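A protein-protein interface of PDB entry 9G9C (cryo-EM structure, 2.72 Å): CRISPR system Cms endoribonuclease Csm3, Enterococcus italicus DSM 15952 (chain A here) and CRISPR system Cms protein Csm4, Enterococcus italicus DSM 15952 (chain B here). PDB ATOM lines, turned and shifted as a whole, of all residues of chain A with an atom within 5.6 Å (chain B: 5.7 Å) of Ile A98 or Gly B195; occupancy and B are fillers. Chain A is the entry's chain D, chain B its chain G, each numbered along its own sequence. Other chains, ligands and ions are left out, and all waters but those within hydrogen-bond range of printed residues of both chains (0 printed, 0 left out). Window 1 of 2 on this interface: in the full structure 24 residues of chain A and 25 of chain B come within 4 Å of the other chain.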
ATOM      1  N   GLY A  48     -21.825  -0.739  16.538  1.00  0.00           N
ATOM      2  CA  GLY A  48     -22.626  -0.276  17.654  1.00  0.00           C
ATOM      3  C   GLY A  48     -23.732   0.678  17.269  1.00  0.00           C
ATOM      4  O   GLY A  48     -24.613   0.944  18.093  1.00  0.00           O
ATOM      5  N   SER A  49     -23.706   1.198  16.042  1.00  0.00           N
ATOM      6  CA  SER A  49     -24.777   2.047  15.548  1.00  0.00           C
ATOM      7  C   SER A  49     -25.936   1.248  14.977  1.00  0.00           C
ATOM      8  O   SER A  49     -27.085   1.681  15.094  1.00  0.00           O
ATOM      9  CB  SER A  49     -24.242   3.006  14.481  1.00  0.00           C
ATOM     10  OG  SER A  49     -23.719   2.300  13.372  1.00  0.00           O
ATOM     11  N   ILE A  51     -27.064  -1.791  16.020  1.00  0.00           N
ATOM     12  CA  ILE A  51     -27.857  -2.288  17.140  1.00  0.00           C
ATOM     13  C   ILE A  51     -28.654  -1.153  17.767  1.00  0.00           C
ATOM     14  O   ILE A  51     -29.844  -1.296  18.071  1.00  0.00           O
ATOM     15  CB  ILE A  51     -26.953  -2.974  18.179  1.00  0.00           C
ATOM     16  CG1 ILE A  51     -26.006  -3.962  17.500  1.00  0.00           C
ATOM     17  CG2 ILE A  51     -27.793  -3.676  19.232  1.00  0.00           C
ATOM     18  CD1 ILE A  51     -24.946  -4.518  18.424  1.00  0.00           C
ATOM     19  N   LYS A  52     -28.002  -0.007  17.973  1.00  0.00           N
ATOM     20  CA  LYS A  52     -28.670   1.137  18.581  1.00  0.00           C
ATOM     21  C   LYS A  52     -29.843   1.605  17.730  1.00  0.00           C
ATOM     22  O   LYS A  52     -30.941   1.845  18.244  1.00  0.00           O
ATOM     23  CB  LYS A  52     -27.663   2.269  18.790  1.00  0.00           C
ATOM     24  CG  LYS A  52     -28.239   3.518  19.423  1.00  0.00           C
ATOM     25  CD  LYS A  52     -27.160   4.563  19.642  1.00  0.00           C
ATOM     26  CE  LYS A  52     -27.718   5.802  20.308  1.00  0.00           C
ATOM     27  NZ  LYS A  52     -26.690   6.864  20.447  1.00  0.00           N
ATOM     28  N   MET A  55     -32.737  -1.096  17.745  1.00  0.00           N
ATOM     29  CA  MET A  55     -33.449  -1.059  19.016  1.00  0.00           C
ATOM     30  C   MET A  55     -34.312   0.191  19.124  1.00  0.00           C
ATOM     31  O   MET A  55     -35.465   0.122  19.565  1.00  0.00           O
ATOM     32  CB  MET A  55     -32.454  -1.125  20.174  1.00  0.00           C
ATOM     33  CG  MET A  55     -31.926  -2.520  20.460  1.00  0.00           C
ATOM     34  SD  MET A  55     -30.467  -2.514  21.519  1.00  0.00           S
ATOM     35  CE  MET A  55     -31.187  -2.057  23.092  1.00  0.00           C
ATOM     36  N   PHE A  83     -31.733   7.201  23.853  1.00  0.00           N
ATOM     37  CA  PHE A  83     -30.843   7.193  22.698  1.00  0.00           C
ATOM     38  C   PHE A  83     -30.378   8.589  22.294  1.00  0.00           C
ATOM     39  O   PHE A  83     -29.937   8.783  21.158  1.00  0.00           O
ATOM     40  CB  PHE A  83     -31.521   6.502  21.517  1.00  0.00           C
ATOM     41  CG  PHE A  83     -32.042   5.132  21.833  1.00  0.00           C
ATOM     42  CD1 PHE A  83     -31.205   4.031  21.787  1.00  0.00           C
ATOM     43  CD2 PHE A  83     -33.372   4.945  22.174  1.00  0.00           C
ATOM     44  CE1 PHE A  83     -31.682   2.771  22.078  1.00  0.00           C
ATOM     45  CE2 PHE A  83     -33.854   3.687  22.466  1.00  0.00           C
ATOM     46  CZ  PHE A  83     -33.007   2.598  22.418  1.00  0.00           C
ATOM     47  N   LEU A  96     -27.890   5.152  26.659  1.00  0.00           N
ATOM     48  CA  LEU A  96     -27.412   3.884  26.128  1.00  0.00           C
ATOM     49  C   LEU A  96     -26.217   4.126  25.215  1.00  0.00           C
ATOM     50  O   LEU A  96     -26.353   4.755  24.160  1.00  0.00           O
ATOM     51  CB  LEU A  96     -28.521   3.162  25.367  1.00  0.00           C
ATOM     52  CG  LEU A  96     -29.489   2.313  26.187  1.00  0.00           C
ATOM     53  CD1 LEU A  96     -30.457   1.593  25.270  1.00  0.00           C
ATOM     54  CD2 LEU A  96     -28.727   1.327  27.051  1.00  0.00           C
ATOM     55  N   GLN A  97     -25.064   3.582  25.630  1.00  0.00           N
ATOM     56  CA  GLN A  97     -23.824   3.656  24.817  1.00  0.00           C
ATOM     57  C   GLN A  97     -23.506   2.226  24.356  1.00  0.00           C
ATOM     58  O   GLN A  97     -22.773   1.527  25.088  1.00  0.00           O
ATOM     59  CB  GLN A  97     -22.696   4.263  25.647  1.00  0.00           C
ATOM     60  CG  GLN A  97     -23.005   5.647  26.204  1.00  0.00           C
ATOM     61  CD  GLN A  97     -21.768   6.361  26.700  1.00  0.00           C
ATOM     62  OE1 GLN A  97     -20.654   5.833  26.630  1.00  0.00           O
ATOM     63  NE2 GLN A  97     -21.948   7.574  27.199  1.00  0.00           N
ATOM     64  N   ILE A  98     -24.013   1.817  23.193  1.00  0.00           N
ATOM     65  CA  ILE A  98     -23.877   0.461  22.677  1.00  0.00           C
ATOM     66  C   ILE A  98     -22.646   0.425  21.785  1.00  0.00           C
ATOM     67  O   ILE A  98     -22.546   1.191  20.820  1.00  0.00           O
ATOM     68  CB  ILE A  98     -25.134   0.025  21.910  1.00  0.00           C
ATOM     69  CG1 ILE A  98     -26.374   0.196  22.790  1.00  0.00           C
ATOM     70  CG2 ILE A  98     -25.001  -1.415  21.440  1.00  0.00           C
ATOM     71  CD1 ILE A  98     -27.670  -0.100  22.084  1.00  0.00           C
ATOM     72  N   SER A  99     -21.709  -0.459  22.107  1.00  0.00           N
ATOM     73  CA  SER A  99     -20.451  -0.542  21.385  1.00  0.00           C
ATOM     74  C   SER A  99     -20.541  -1.571  20.262  1.00  0.00           C
ATOM     75  O   SER A  99     -21.477  -2.367  20.182  1.00  0.00           O
ATOM     76  CB  SER A  99     -19.314  -0.895  22.339  1.00  0.00           C
ATOM     77  OG  SER A  99     -19.215   0.061  23.378  1.00  0.00           O
ATOM     78  N   ASP A 100     -19.544  -1.539  19.381  1.00  0.00           N
ATOM     79  CA  ASP A 100     -19.475  -2.513  18.301  1.00  0.00           C
ATOM     80  C   ASP A 100     -19.298  -3.916  18.866  1.00  0.00           C
ATOM     81  O   ASP A 100     -18.504  -4.140  19.783  1.00  0.00           O
ATOM     82  CB  ASP A 100     -18.320  -2.180  17.355  1.00  0.00           C
ATOM     83  CG  ASP A 100     -18.413  -0.778  16.787  1.00  0.00           C
ATOM     84  OD1 ASP A 100     -19.541  -0.283  16.595  1.00  0.00           O
ATOM     85  OD2 ASP A 100     -17.353  -0.170  16.530  1.00  0.00           O
ATOM     86  N   HIS A 151     -21.428  -5.216  24.108  1.00  0.00           N
ATOM     87  CA  HIS A 151     -21.147  -4.412  25.287  1.00  0.00           C
ATOM     88  C   HIS A 151     -22.083  -3.215  25.282  1.00  0.00           C
ATOM     89  O   HIS A 151     -22.223  -2.542  24.257  1.00  0.00           O
ATOM     90  CB  HIS A 151     -19.682  -3.962  25.280  1.00  0.00           C
ATOM     91  CG  HIS A 151     -19.287  -3.138  26.462  1.00  0.00           C
ATOM     92  ND1 HIS A 151     -18.601  -3.660  27.536  1.00  0.00           N
ATOM     93  CD2 HIS A 151     -19.457  -1.822  26.729  1.00  0.00           C
ATOM     94  CE1 HIS A 151     -18.376  -2.705  28.419  1.00  0.00           C
ATOM     95  NE2 HIS A 151     -18.886  -1.580  27.954  1.00  0.00           N
ATOM     96  N   ILE A 152     -22.731  -2.956  26.415  1.00  0.00           N
ATOM     97  CA  ILE A 152     -23.665  -1.847  26.546  1.00  0.00           C
ATOM     98  C   ILE A 152     -23.373  -1.128  27.854  1.00  0.00           C
ATOM     99  O   ILE A 152     -23.080  -1.767  28.869  1.00  0.00           O
ATOM    100  CB  ILE A 152     -25.130  -2.333  26.498  1.00  0.00           C
ATOM    101  CG1 ILE A 152     -25.468  -2.881  25.112  1.00  0.00           C
ATOM    102  CG2 ILE A 152     -26.088  -1.214  26.861  1.00  0.00           C
ATOM    103  CD1 ILE A 152     -26.925  -3.240  24.937  1.00  0.00           C
ATOM    104  N   ILE A 153     -23.426   0.208  27.813  1.00  0.00           N
ATOM    105  CA  ILE A 153     -23.230   1.026  29.047  1.00  0.00           C
ATOM    106  C   ILE A 153     -24.468   1.914  29.226  1.00  0.00           C
ATOM    107  O   ILE A 153     -24.829   2.614  28.264  1.00  0.00           O
ATOM    108  CB  ILE A 153     -21.935   1.860  28.995  1.00  0.00           C
ATOM    109  CG1 ILE A 153     -20.698   0.986  29.139  1.00  0.00           C
ATOM    110  CG2 ILE A 153     -21.950   2.967  30.049  1.00  0.00           C
ATOM    111  CD1 ILE A 153     -20.531   0.390  30.523  1.00  0.00           C
ATOM    112  N   SER B  15     -12.877  -0.714  20.912  1.00  0.00           N
ATOM    113  CA  SER B  15     -13.584  -0.445  19.673  1.00  0.00           C
ATOM    114  C   SER B  15     -12.882   0.683  18.930  1.00  0.00           C
ATOM    115  O   SER B  15     -12.121   1.450  19.532  1.00  0.00           O
ATOM    116  CB  SER B  15     -15.047  -0.064  19.949  1.00  0.00           C
ATOM    117  OG  SER B  15     -15.132   1.008  20.870  1.00  0.00           O
ATOM    118  N   PRO B  16     -13.094   0.804  17.619  1.00  0.00           N
ATOM    119  CA  PRO B  16     -12.471   1.905  16.879  1.00  0.00           C
ATOM    120  C   PRO B  16     -12.927   3.256  17.410  1.00  0.00           C
ATOM    121  O   PRO B  16     -14.011   3.393  17.976  1.00  0.00           O
ATOM    122  CB  PRO B  16     -12.940   1.680  15.436  1.00  0.00           C
ATOM    123  CG  PRO B  16     -14.107   0.756  15.541  1.00  0.00           C
ATOM    124  CD  PRO B  16     -13.821  -0.109  16.723  1.00  0.00           C
ATOM    125  N   LYS B 191     -18.806  10.328  17.843  1.00  0.00           N
ATOM    126  CA  LYS B 191     -19.664   9.117  17.687  1.00  0.00           C
ATOM    127  C   LYS B 191     -19.517   8.212  18.916  1.00  0.00           C
ATOM    128  O   LYS B 191     -19.900   7.035  18.825  1.00  0.00           O
ATOM    129  CB  LYS B 191     -19.473   8.413  16.336  1.00  0.00           C
ATOM    130  CG  LYS B 191     -20.155   9.141  15.191  1.00  0.00           C
ATOM    131  CD  LYS B 191     -21.491   9.714  15.646  1.00  0.00           C
ATOM    132  CE  LYS B 191     -22.206  10.507  14.603  1.00  0.00           C
ATOM    133  NZ  LYS B 191     -22.757   9.647  13.554  1.00  0.00           N
ATOM    134  N   ARG B 192     -18.963   8.735  20.010  1.00  0.00           N
ATOM    135  CA  ARG B 192     -18.974   7.943  21.268  1.00  0.00           C
ATOM    136  C   ARG B 192     -20.462   7.860  21.630  1.00  0.00           C
ATOM    137  O   ARG B 192     -21.158   8.854  21.311  1.00  0.00           O
ATOM    138  CB  ARG B 192     -18.124   8.565  22.380  1.00  0.00           C
ATOM    139  CG  ARG B 192     -18.527   9.986  22.739  1.00  0.00           C
ATOM    140  CD  ARG B 192     -17.966  10.390  24.082  1.00  0.00           C
ATOM    141  NE  ARG B 192     -18.743  11.506  24.629  1.00  0.00           N
ATOM    142  CZ  ARG B 192     -19.431  11.440  25.757  1.00  0.00           C
ATOM    143  NH1 ARG B 192     -19.524  10.294  26.406  1.00  0.00           N
ATOM    144  NH2 ARG B 192     -20.020  12.521  26.234  1.00  0.00           N
ATOM    145  N   SER B 193     -20.939   6.745  22.190  1.00  0.00           N
ATOM    146  CA  SER B 193     -22.397   6.539  22.442  1.00  0.00           C
ATOM    147  C   SER B 193     -23.066   6.095  21.134  1.00  0.00           C
ATOM    148  O   SER B 193     -24.307   6.041  21.108  1.00  0.00           O
ATOM    149  CB  SER B 193     -23.106   7.727  23.057  1.00  0.00           C
ATOM    150  OG  SER B 193     -23.728   8.519  22.054  1.00  0.00           O
ATOM    151  N   ALA B 194     -22.279   5.817  20.090  1.00  0.00           N
ATOM    152  CA  ALA B 194     -22.818   5.264  18.823  1.00  0.00           C
ATOM    153  C   ALA B 194     -21.877   4.148  18.368  1.00  0.00           C
ATOM    154  O   ALA B 194     -21.861   3.835  17.163  1.00  0.00           O
ATOM    155  CB  ALA B 194     -22.993   6.343  17.784  1.00  0.00           C
ATOM    156  N   GLY B 195     -21.083   3.598  19.295  1.00  0.00           N
ATOM    157  CA  GLY B 195     -20.239   2.456  18.997  1.00  0.00           C
ATOM    158  C   GLY B 195     -18.747   2.706  19.026  1.00  0.00           C
ATOM    159  O   GLY B 195     -17.983   1.766  18.780  1.00  0.00           O
ATOM    160  N   TYR B 196     -18.314   3.923  19.357  1.00  0.00           N
ATOM    161  CA  TYR B 196     -16.861   4.208  19.227  1.00  0.00           C
ATOM    162  C   TYR B 196     -16.230   4.784  20.483  1.00  0.00           C
ATOM    163  O   TYR B 196     -16.954   5.324  21.339  1.00  0.00           O
ATOM    164  CB  TYR B 196     -16.687   5.232  18.101  1.00  0.00           C
ATOM    165  CG  TYR B 196     -17.013   4.741  16.699  1.00  0.00           C
ATOM    166  CD1 TYR B 196     -16.065   4.063  15.949  1.00  0.00           C
ATOM    167  CD2 TYR B 196     -18.249   4.981  16.116  1.00  0.00           C
ATOM    168  CE1 TYR B 196     -16.339   3.610  14.673  1.00  0.00           C
ATOM    169  CE2 TYR B 196     -18.536   4.540  14.836  1.00  0.00           C
ATOM    170  CZ  TYR B 196     -17.576   3.854  14.113  1.00  0.00           C
ATOM    171  OH  TYR B 196     -17.817   3.402  12.852  1.00  0.00           O
ATOM    172  N   GLY B 197     -14.906   4.663  20.601  1.00  0.00           N
ATOM    173  CA  GLY B 197     -14.172   5.324  21.697  1.00  0.00           C
ATOM    174  C   GLY B 197     -14.111   4.602  23.026  1.00  0.00           C
ATOM    175  O   GLY B 197     -13.488   5.171  23.940  1.00  0.00           O
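The side-chain amino group (NZ) of Lys A52 is in hydrogen-bond range of the backbone carbonyl oxygen (O) of Ser B193, 2.6 Å away.
N of Gly B195 lies close to O of Ile A98 (3.2 Å).
The backbone carbonyl oxygen (O) of Ala B194 is in hydrogen-bond range of the backbone NH (N) of Ser A49.
The side-chain carboxylate (OD2) of Asp A100 sits close to the backbone carbonyl oxygen (O) of Gly B195.
Of the 14 printed residues of chain A, 8 touch a printed residue of chain B.
Along chain A the printed residues that touch a printed residue of chain B span positions 48 to 100.
Among the printed residues, 12 pairs touch across the chains.
Printed residues of chain B within 4 Å of Ser A49: Ala B194 (3.4 Å).
Met A55 touches none of the printed residues of chain B.
Printed residues of chain B within 4 Å of Leu A96: Ser B193 (3.9 Å).
Of the printed residues of chain B, Gln A97 touches Arg B192 (3.7 Å) and Ser B193 (3.8 Å).
Of chain B, only Ala B194 and Gly B195 come within 4 Å of Ile A98.
Ile A153 touches none of the printed residues of chain B.
Printed residues of chain A within 4 Å of Pro B16: Asp A100 (3.5 Å).
Printed residues of chain A within 4 Å of Ser B193: Lys A52 (2.6 Å), Leu A96 (3.9 Å) and Gln A97 (3.8 Å).
Of chain A, only Gly A48, Ile A98, Ser A99 and Asp A100 come within 4 Å of Gly B195.
The nearest residue of chain A that does not touch Gly B195 is Ser A49 (4.7 Å).
The backbone NH of Gln A97 sits at hydrogen-bond distance from the backbone carbonyl oxygen of Ile A153, 2.8 Å away.
The backbone NH (N) of Gly B197 sits at hydrogen-bond distance from the backbone carbonyl oxygen (O) of Pro B16, at 3.1 Å.
O of His A151 is in hydrogen-bond range of N of Ser A99, 3.0 Å away.
Gly A48 touches Ala B194 (C to O, 3.7 Å).
Gly B195 touches Gly A48 (CA to CA, 3.9 Å).
O of Leu A96 touches O of Ser B193, at 3.9 Å.
Gln A97 touches Arg B192 (NE2 to NH1, 3.7 Å).
CG of Gln A97 touches CB of Ser B193 (3.8 Å).
Ala B194 touches Ile A98.
Gly B195 touches Ser A99 (CA to CA, 3.8 Å).
Asp A100 touches Pro B16.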
